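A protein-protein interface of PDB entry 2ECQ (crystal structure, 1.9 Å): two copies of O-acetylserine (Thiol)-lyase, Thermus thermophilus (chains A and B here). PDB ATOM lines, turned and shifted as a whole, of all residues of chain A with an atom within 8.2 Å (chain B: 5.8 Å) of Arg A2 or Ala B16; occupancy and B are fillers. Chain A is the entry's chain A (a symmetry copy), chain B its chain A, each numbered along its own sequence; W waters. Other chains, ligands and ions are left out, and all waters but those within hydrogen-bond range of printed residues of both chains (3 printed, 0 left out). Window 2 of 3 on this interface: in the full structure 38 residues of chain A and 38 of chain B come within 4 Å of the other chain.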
ATOM      1  N   MET A   1     -12.049  23.683 -14.096  1.00  0.00           N
ATOM      2  CA  MET A   1     -10.574  23.737 -14.281  1.00  0.00           C
ATOM      3  C   MET A   1     -10.227  24.811 -15.303  1.00  0.00           C
ATOM      4  O   MET A   1     -10.977  25.041 -16.246  1.00  0.00           O
ATOM      5  CB  MET A   1     -10.057  22.377 -14.765  1.00  0.00           C
ATOM      6  CG  MET A   1      -8.548  22.303 -14.931  1.00  0.00           C
ATOM      7  SD  MET A   1      -7.965  20.701 -15.538  1.00  0.00           S
ATOM      8  CE  MET A   1      -7.996  20.975 -17.298  1.00  0.00           C
ATOM      9  N   ARG A   2      -9.095  25.479 -15.111  1.00  0.00           N
ATOM     10  CA  ARG A   2      -8.677  26.508 -16.050  1.00  0.00           C
ATOM     11  C   ARG A   2      -7.506  25.998 -16.882  1.00  0.00           C
ATOM     12  O   ARG A   2      -6.953  24.938 -16.588  1.00  0.00           O
ATOM     13  CB  ARG A   2      -8.338  27.797 -15.296  1.00  0.00           C
ATOM     14  CG  ARG A   2      -9.565  28.342 -14.571  1.00  0.00           C
ATOM     15  CD  ARG A   2      -9.383  29.750 -14.071  1.00  0.00           C
ATOM     16  NE  ARG A   2     -10.596  30.246 -13.420  1.00  0.00           N
ATOM     17  CZ  ARG A   2     -10.740  31.483 -12.956  1.00  0.00           C
ATOM     18  NH1 ARG A   2      -9.746  32.349 -13.077  1.00  0.00           N
ATOM     19  NH2 ARG A   2     -11.875  31.852 -12.370  1.00  0.00           N
ATOM     20  N   VAL A   3      -7.134  26.744 -17.918  1.00  0.00           N
ATOM     21  CA  VAL A   3      -6.063  26.307 -18.810  1.00  0.00           C
ATOM     22  C   VAL A   3      -4.770  25.878 -18.116  1.00  0.00           C
ATOM     23  O   VAL A   3      -4.137  24.913 -18.543  1.00  0.00           O
ATOM     24  CB  VAL A   3      -5.746  27.386 -19.881  1.00  0.00           C
ATOM     25  CG1 VAL A   3      -5.018  28.561 -19.252  1.00  0.00           C
ATOM     26  CG2 VAL A   3      -4.923  26.768 -21.015  1.00  0.00           C
ATOM     27  N   GLU A   4      -4.376  26.575 -17.052  1.00  0.00           N
ATOM     28  CA  GLU A   4      -3.152  26.205 -16.341  1.00  0.00           C
ATOM     29  C   GLU A   4      -3.264  24.783 -15.801  1.00  0.00           C
ATOM     30  O   GLU A   4      -2.258  24.108 -15.589  1.00  0.00           O
ATOM     31  CB  GLU A   4      -2.857  27.179 -15.188  1.00  0.00           C
ATOM     32  CG  GLU A   4      -4.011  27.383 -14.217  1.00  0.00           C
ATOM     33  CD  GLU A   4      -4.845  28.602 -14.556  1.00  0.00           C
ATOM     34  OE1 GLU A   4      -4.996  28.908 -15.761  1.00  0.00           O
ATOM     35  OE2 GLU A   4      -5.356  29.251 -13.618  1.00  0.00           O
ATOM     36  N   GLY A   5      -4.495  24.331 -15.579  1.00  0.00           N
ATOM     37  CA  GLY A   5      -4.701  22.981 -15.083  1.00  0.00           C
ATOM     38  C   GLY A   5      -4.535  21.929 -16.170  1.00  0.00           C
ATOM     39  O   GLY A   5      -4.421  20.737 -15.878  1.00  0.00           O
ATOM     40  N   ALA A   6      -4.513  22.367 -17.426  1.00  0.00           N
ATOM     41  CA  ALA A   6      -4.360  21.454 -18.558  1.00  0.00           C
ATOM     42  C   ALA A   6      -2.893  21.255 -18.945  1.00  0.00           C
ATOM     43  O   ALA A   6      -2.585  20.592 -19.942  1.00  0.00           O
ATOM     44  CB  ALA A   6      -5.142  21.981 -19.753  1.00  0.00           C
ATOM     45  N   ILE A   7      -1.993  21.834 -18.157  1.00  0.00           N
ATOM     46  CA  ILE A   7      -0.558  21.725 -18.410  1.00  0.00           C
ATOM     47  C   ILE A   7       0.015  20.412 -17.878  1.00  0.00           C
ATOM     48  O   ILE A   7      -0.326  19.982 -16.777  1.00  0.00           O
ATOM     49  CB  ILE A   7       0.216  22.885 -17.735  1.00  0.00           C
ATOM     50  CG1 ILE A   7      -0.166  24.221 -18.379  1.00  0.00           C
ATOM     51  CG2 ILE A   7       1.722  22.646 -17.843  1.00  0.00           C
ATOM     52  CD1 ILE A   7       0.453  25.428 -17.688  1.00  0.00           C
ATOM     53  N   PRO A  35      -1.139  23.202 -23.612  1.00  0.00           N
ATOM     54  CA  PRO A  35      -2.018  24.277 -24.088  1.00  0.00           C
ATOM     55  C   PRO A  35      -1.304  25.478 -24.696  1.00  0.00           C
ATOM     56  O   PRO A  35      -1.847  26.146 -25.576  1.00  0.00           O
ATOM     57  CB  PRO A  35      -2.836  24.640 -22.844  1.00  0.00           C
ATOM     58  CG  PRO A  35      -1.936  24.255 -21.708  1.00  0.00           C
ATOM     59  CD  PRO A  35      -1.349  22.946 -22.176  1.00  0.00           C
ATOM     60  N   PRO A  59      -3.472  36.511  -8.034  1.00  0.00           N
ATOM     61  CA  PRO A  59      -4.260  36.494  -9.270  1.00  0.00           C
ATOM     62  C   PRO A  59      -5.457  37.444  -9.330  1.00  0.00           C
ATOM     63  O   PRO A  59      -6.092  37.728  -8.315  1.00  0.00           O
ATOM     64  CB  PRO A  59      -4.663  35.028  -9.390  1.00  0.00           C
ATOM     65  CG  PRO A  59      -4.838  34.625  -7.965  1.00  0.00           C
ATOM     66  CD  PRO A  59      -3.611  35.233  -7.313  1.00  0.00           C
ATOM     67  N   GLY A  60      -5.741  37.934 -10.536  1.00  0.00           N
ATOM     68  CA  GLY A  60      -6.861  38.838 -10.745  1.00  0.00           C
ATOM     69  C   GLY A  60      -6.591  40.256 -10.286  1.00  0.00           C
ATOM     70  O   GLY A  60      -7.501  41.084 -10.225  1.00  0.00           O
ATOM     71  N   ILE A  80      -0.710  32.185 -19.257  1.00  0.00           N
ATOM     72  CA  ILE A  80      -0.980  32.224 -17.824  1.00  0.00           C
ATOM     73  C   ILE A  80      -1.452  33.606 -17.363  1.00  0.00           C
ATOM     74  O   ILE A  80      -2.369  33.716 -16.546  1.00  0.00           O
ATOM     75  CB  ILE A  80       0.274  31.826 -17.005  1.00  0.00           C
ATOM     76  CG1 ILE A  80       0.767  30.439 -17.427  1.00  0.00           C
ATOM     77  CG2 ILE A  80      -0.059  31.815 -15.513  1.00  0.00           C
ATOM     78  CD1 ILE A  80      -0.208  29.319 -17.144  1.00  0.00           C
ATOM     79  N   ALA A  82      -3.011  35.800 -19.132  1.00  0.00           N
ATOM     80  CA  ALA A  82      -4.358  36.014 -19.644  1.00  0.00           C
ATOM     81  C   ALA A  82      -5.355  35.300 -18.737  1.00  0.00           C
ATOM     82  O   ALA A  82      -6.373  35.868 -18.341  1.00  0.00           O
ATOM     83  CB  ALA A  82      -4.474  35.484 -21.070  1.00  0.00           C
ATOM     84  N   SER A  83      -5.043  34.059 -18.388  1.00  0.00           N
ATOM     85  CA  SER A  83      -5.929  33.278 -17.537  1.00  0.00           C
ATOM     86  C   SER A  83      -6.049  33.781 -16.102  1.00  0.00           C
ATOM     87  O   SER A  83      -7.139  33.783 -15.534  1.00  0.00           O
ATOM     88  CB  SER A  83      -5.480  31.817 -17.505  1.00  0.00           C
ATOM     89  OG  SER A  83      -6.284  31.069 -16.604  1.00  0.00           O
ATOM     90  N   ARG A  84      -4.938  34.215 -15.517  1.00  0.00           N
ATOM     91  CA  ARG A  84      -4.969  34.656 -14.131  1.00  0.00           C
ATOM     92  C   ARG A  84      -5.079  36.153 -13.884  1.00  0.00           C
ATOM     93  O   ARG A  84      -4.975  36.604 -12.747  1.00  0.00           O
ATOM     94  CB  ARG A  84      -3.771  34.066 -13.392  1.00  0.00           C
ATOM     95  CG  ARG A  84      -3.766  32.539 -13.450  1.00  0.00           C
ATOM     96  CD  ARG A  84      -2.641  31.934 -12.634  1.00  0.00           C
ATOM     97  NE  ARG A  84      -2.889  31.963 -11.193  1.00  0.00           N
ATOM     98  CZ  ARG A  84      -3.796  31.223 -10.561  1.00  0.00           C
ATOM     99  NH1 ARG A  84      -4.571  30.381 -11.235  1.00  0.00           N
ATOM    100  NH2 ARG A  84      -3.910  31.304  -9.239  1.00  0.00           N
ATOM    101  N   GLY A  85      -5.296  36.917 -14.947  1.00  0.00           N
ATOM    102  CA  GLY A  85      -5.473  38.348 -14.804  1.00  0.00           C
ATOM    103  C   GLY A  85      -4.278  39.230 -14.494  1.00  0.00           C
ATOM    104  O   GLY A  85      -4.380  40.141 -13.668  1.00  0.00           O
ATOM    105  N   VAL B  13     -11.954  22.551 -19.890  1.00  0.00           N
ATOM    106  CA  VAL B  13     -11.784  23.712 -19.029  1.00  0.00           C
ATOM    107  C   VAL B  13     -13.091  24.485 -18.890  1.00  0.00           C
ATOM    108  O   VAL B  13     -13.911  24.502 -19.809  1.00  0.00           O
ATOM    109  CB  VAL B  13     -10.700  24.662 -19.590  1.00  0.00           C
ATOM    110  CG1 VAL B  13      -9.358  23.946 -19.636  1.00  0.00           C
ATOM    111  CG2 VAL B  13     -11.093  25.139 -20.984  1.00  0.00           C
ATOM    112  N   ARG B  14     -13.284  25.120 -17.737  1.00  0.00           N
ATOM    113  CA  ARG B  14     -14.494  25.903 -17.505  1.00  0.00           C
ATOM    114  C   ARG B  14     -14.206  27.384 -17.723  1.00  0.00           C
ATOM    115  O   ARG B  14     -13.271  27.934 -17.135  1.00  0.00           O
ATOM    116  CB  ARG B  14     -15.012  25.693 -16.078  1.00  0.00           C
ATOM    117  CG  ARG B  14     -16.260  26.511 -15.774  1.00  0.00           C
ATOM    118  CD  ARG B  14     -16.735  26.347 -14.334  1.00  0.00           C
ATOM    119  NE  ARG B  14     -17.810  27.294 -14.047  1.00  0.00           N
ATOM    120  CZ  ARG B  14     -18.411  27.426 -12.868  1.00  0.00           C
ATOM    121  NH1 ARG B  14     -18.050  26.669 -11.842  1.00  0.00           N
ATOM    122  NH2 ARG B  14     -19.373  28.327 -12.717  1.00  0.00           N
ATOM    123  N   LEU B  15     -15.008  28.027 -18.568  1.00  0.00           N
ATOM    124  CA  LEU B  15     -14.827  29.445 -18.854  1.00  0.00           C
ATOM    125  C   LEU B  15     -15.167  30.247 -17.603  1.00  0.00           C
ATOM    126  O   LEU B  15     -16.068  29.873 -16.851  1.00  0.00           O
ATOM    127  CB  LEU B  15     -15.727  29.869 -20.015  1.00  0.00           C
ATOM    128  CG  LEU B  15     -15.485  29.116 -21.329  1.00  0.00           C
ATOM    129  CD1 LEU B  15     -16.411  29.665 -22.408  1.00  0.00           C
ATOM    130  CD2 LEU B  15     -14.024  29.267 -21.751  1.00  0.00           C
ATOM    131  N   ALA B  16     -14.458  31.354 -17.391  1.00  0.00           N
ATOM    132  CA  ALA B  16     -14.682  32.172 -16.202  1.00  0.00           C
ATOM    133  C   ALA B  16     -14.765  33.679 -16.442  1.00  0.00           C
ATOM    134  O   ALA B  16     -15.256  34.415 -15.584  1.00  0.00           O
ATOM    135  CB  ALA B  16     -13.592  31.875 -15.178  1.00  0.00           C
ATOM    136  N   LYS B  17     -14.292  34.141 -17.596  1.00  0.00           N
ATOM    137  CA  LYS B  17     -14.309  35.572 -17.896  1.00  0.00           C
ATOM    138  C   LYS B  17     -15.326  36.019 -18.940  1.00  0.00           C
ATOM    139  O   LYS B  17     -15.965  37.057 -18.773  1.00  0.00           O
ATOM    140  CB  LYS B  17     -12.915  36.043 -18.332  1.00  0.00           C
ATOM    141  CG  LYS B  17     -11.872  36.090 -17.217  1.00  0.00           C
ATOM    142  CD  LYS B  17     -11.497  34.694 -16.746  1.00  0.00           C
ATOM    143  CE  LYS B  17     -10.275  34.723 -15.856  1.00  0.00           C
ATOM    144  NZ  LYS B  17      -9.095  35.303 -16.557  1.00  0.00           N
ATOM    145  N   VAL B  18     -15.469  35.260 -20.022  1.00  0.00           N
ATOM    146  CA  VAL B  18     -16.420  35.630 -21.070  1.00  0.00           C
ATOM    147  C   VAL B  18     -17.852  35.259 -20.702  1.00  0.00           C
ATOM    148  O   VAL B  18     -18.792  35.604 -21.416  1.00  0.00           O
ATOM    149  CB  VAL B  18     -16.073  34.967 -22.427  1.00  0.00           C
ATOM    150  CG1 VAL B  18     -14.683  35.403 -22.878  1.00  0.00           C
ATOM    151  CG2 VAL B  18     -16.158  33.450 -22.312  1.00  0.00           C
ATOM    152  N   VAL B  19     -18.016  34.554 -19.589  1.00  0.00           N
ATOM    153  CA  VAL B  19     -19.343  34.161 -19.137  1.00  0.00           C
ATOM    154  C   VAL B  19     -19.860  35.179 -18.128  1.00  0.00           C
ATOM    155  O   VAL B  19     -19.088  35.964 -17.575  1.00  0.00           O
ATOM    156  CB  VAL B  19     -19.331  32.765 -18.478  1.00  0.00           C
ATOM    157  CG1 VAL B  19     -19.020  31.699 -19.524  1.00  0.00           C
ATOM    158  CG2 VAL B  19     -18.309  32.723 -17.352  1.00  0.00           C
ATOM    159  N   GLU B 256      -9.146  34.139 -21.219  1.00  0.00           N
ATOM    160  CA  GLU B 256      -9.169  32.789 -20.658  1.00  0.00           C
ATOM    161  C   GLU B 256      -7.844  32.067 -20.899  1.00  0.00           C
ATOM    162  O   GLU B 256      -7.587  31.022 -20.310  1.00  0.00           O
ATOM    163  CB  GLU B 256     -10.296  31.961 -21.291  1.00  0.00           C
ATOM    164  CG  GLU B 256     -11.658  32.649 -21.350  1.00  0.00           C
ATOM    165  CD  GLU B 256     -12.469  32.520 -20.069  1.00  0.00           C
ATOM    166  OE1 GLU B 256     -13.577  33.090 -20.026  1.00  0.00           O
ATOM    167  OE2 GLU B 256     -12.018  31.850 -19.115  1.00  0.00           O
HETATM  168  O   HOH W   1     -13.184  28.355 -14.224  1.00  0.00           O
HETATM  169  O   HOH W   2      -9.197  31.830 -16.906  1.00  0.00           O
HETATM  170  O   HOH W   3      -8.513  29.106 -18.663  1.00  0.00           O
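The backbone NH (N) of Arg B14 lies within hydrogen-bond range of the backbone carbonyl oxygen (O) of Met A1.
NZ of Lys B17 is in hydrogen-bond range of O of Ala A82 (3.3 Å).
O of Ser A83 lies within hydrogen-bond range of NZ of Lys B17 (2.7 Å).
The backbone NH (N) of Ala B16 is in hydrogen-bond range of the side-chain carboxylate (OE2) of Glu B256 (3.0 Å).
OE1 of Glu B256 lies within hydrogen-bond range of N of Lys B17, 2.7 Å away.
OE1 of Glu B256 lies within hydrogen-bond range of N of Val B18, at 2.9 Å.
OE1 of Glu A4 is in hydrogen-bond range of OG of Ser A83.
Among the printed residues, merely in contact across the chains: Met A1 with Val B13 (3.2 Å), Arg A2 with Ala B16 (3.3 Å), Ser A83 with Glu B256 (3.6 Å), Arg A2 with Lys B17 (3.7 Å), Val A3 with Glu B256 (3.7 Å), Arg A2 with Val B13 (3.9 Å) and Val A3 with Val B13 (3.97 Å).
Of chain B, only Val B13 (3.9 Å), Ala B16 (3.3 Å) and Lys B17 (3.7 Å) come within 4 Å of Arg A2.
Printed residues of chain B within 4 Å of Met A1: Val B13 (3.2 Å) and Arg B14 (2.7 Å).
Of the printed residues of chain A, Glu B256 touches Val A3 (3.7 Å) and Ser A83 (3.6 Å).
Of the printed residues of chain A, Lys B17 touches Arg A2, Ala A82 and Ser A83.
Printed residues of chain A within 4 Å of Val B13: Met A1, Arg A2 and Val A3.
The nearest residue of chain A that does not touch Ala B16 is Ser A83 (6.7 Å).
Of the 8 printed residues of chain B, 5 touch a printed residue of chain A.
Printed residues of chain B that touch a printed residue of chain A: Val B13, Arg B14, Ala B16, Lys B17 and Glu B256.
Hydrophobic or aromatic side chains of chain B within 4 Å of the printed part of chain A: Val B13 and Ala B16.
Printed residues of chain A that touch a printed residue of chain B: Met A1, Arg A2, Val A3, Ala A82 and Ser A83.
Among the printed residues, 10 pairs touch across the chains.
Among the printed residues, no Asp or Glu carboxylate lies within 4 Å of a Lys or Arg side-chain nitrogen of the other chain.
No position is printed for both chains.
Of the 10 pairs that touch across the chains among the printed residues, none has its exchanged pair printed and touching as well.
Water W3 lies within hydrogen-bond range of the backbone carbonyl oxygen (O) of Glu B256 and the backbone NH (N) of Val A3.
Water W1 bridges O of Arg B14 (2.9 Å) and NE of Arg A2 (3.3 Å).
Water W2 lies within hydrogen-bond range of the side-chain hydroxyl (OG) of Ser A83 and the side-chain amino group (NZ) of Lys B17.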
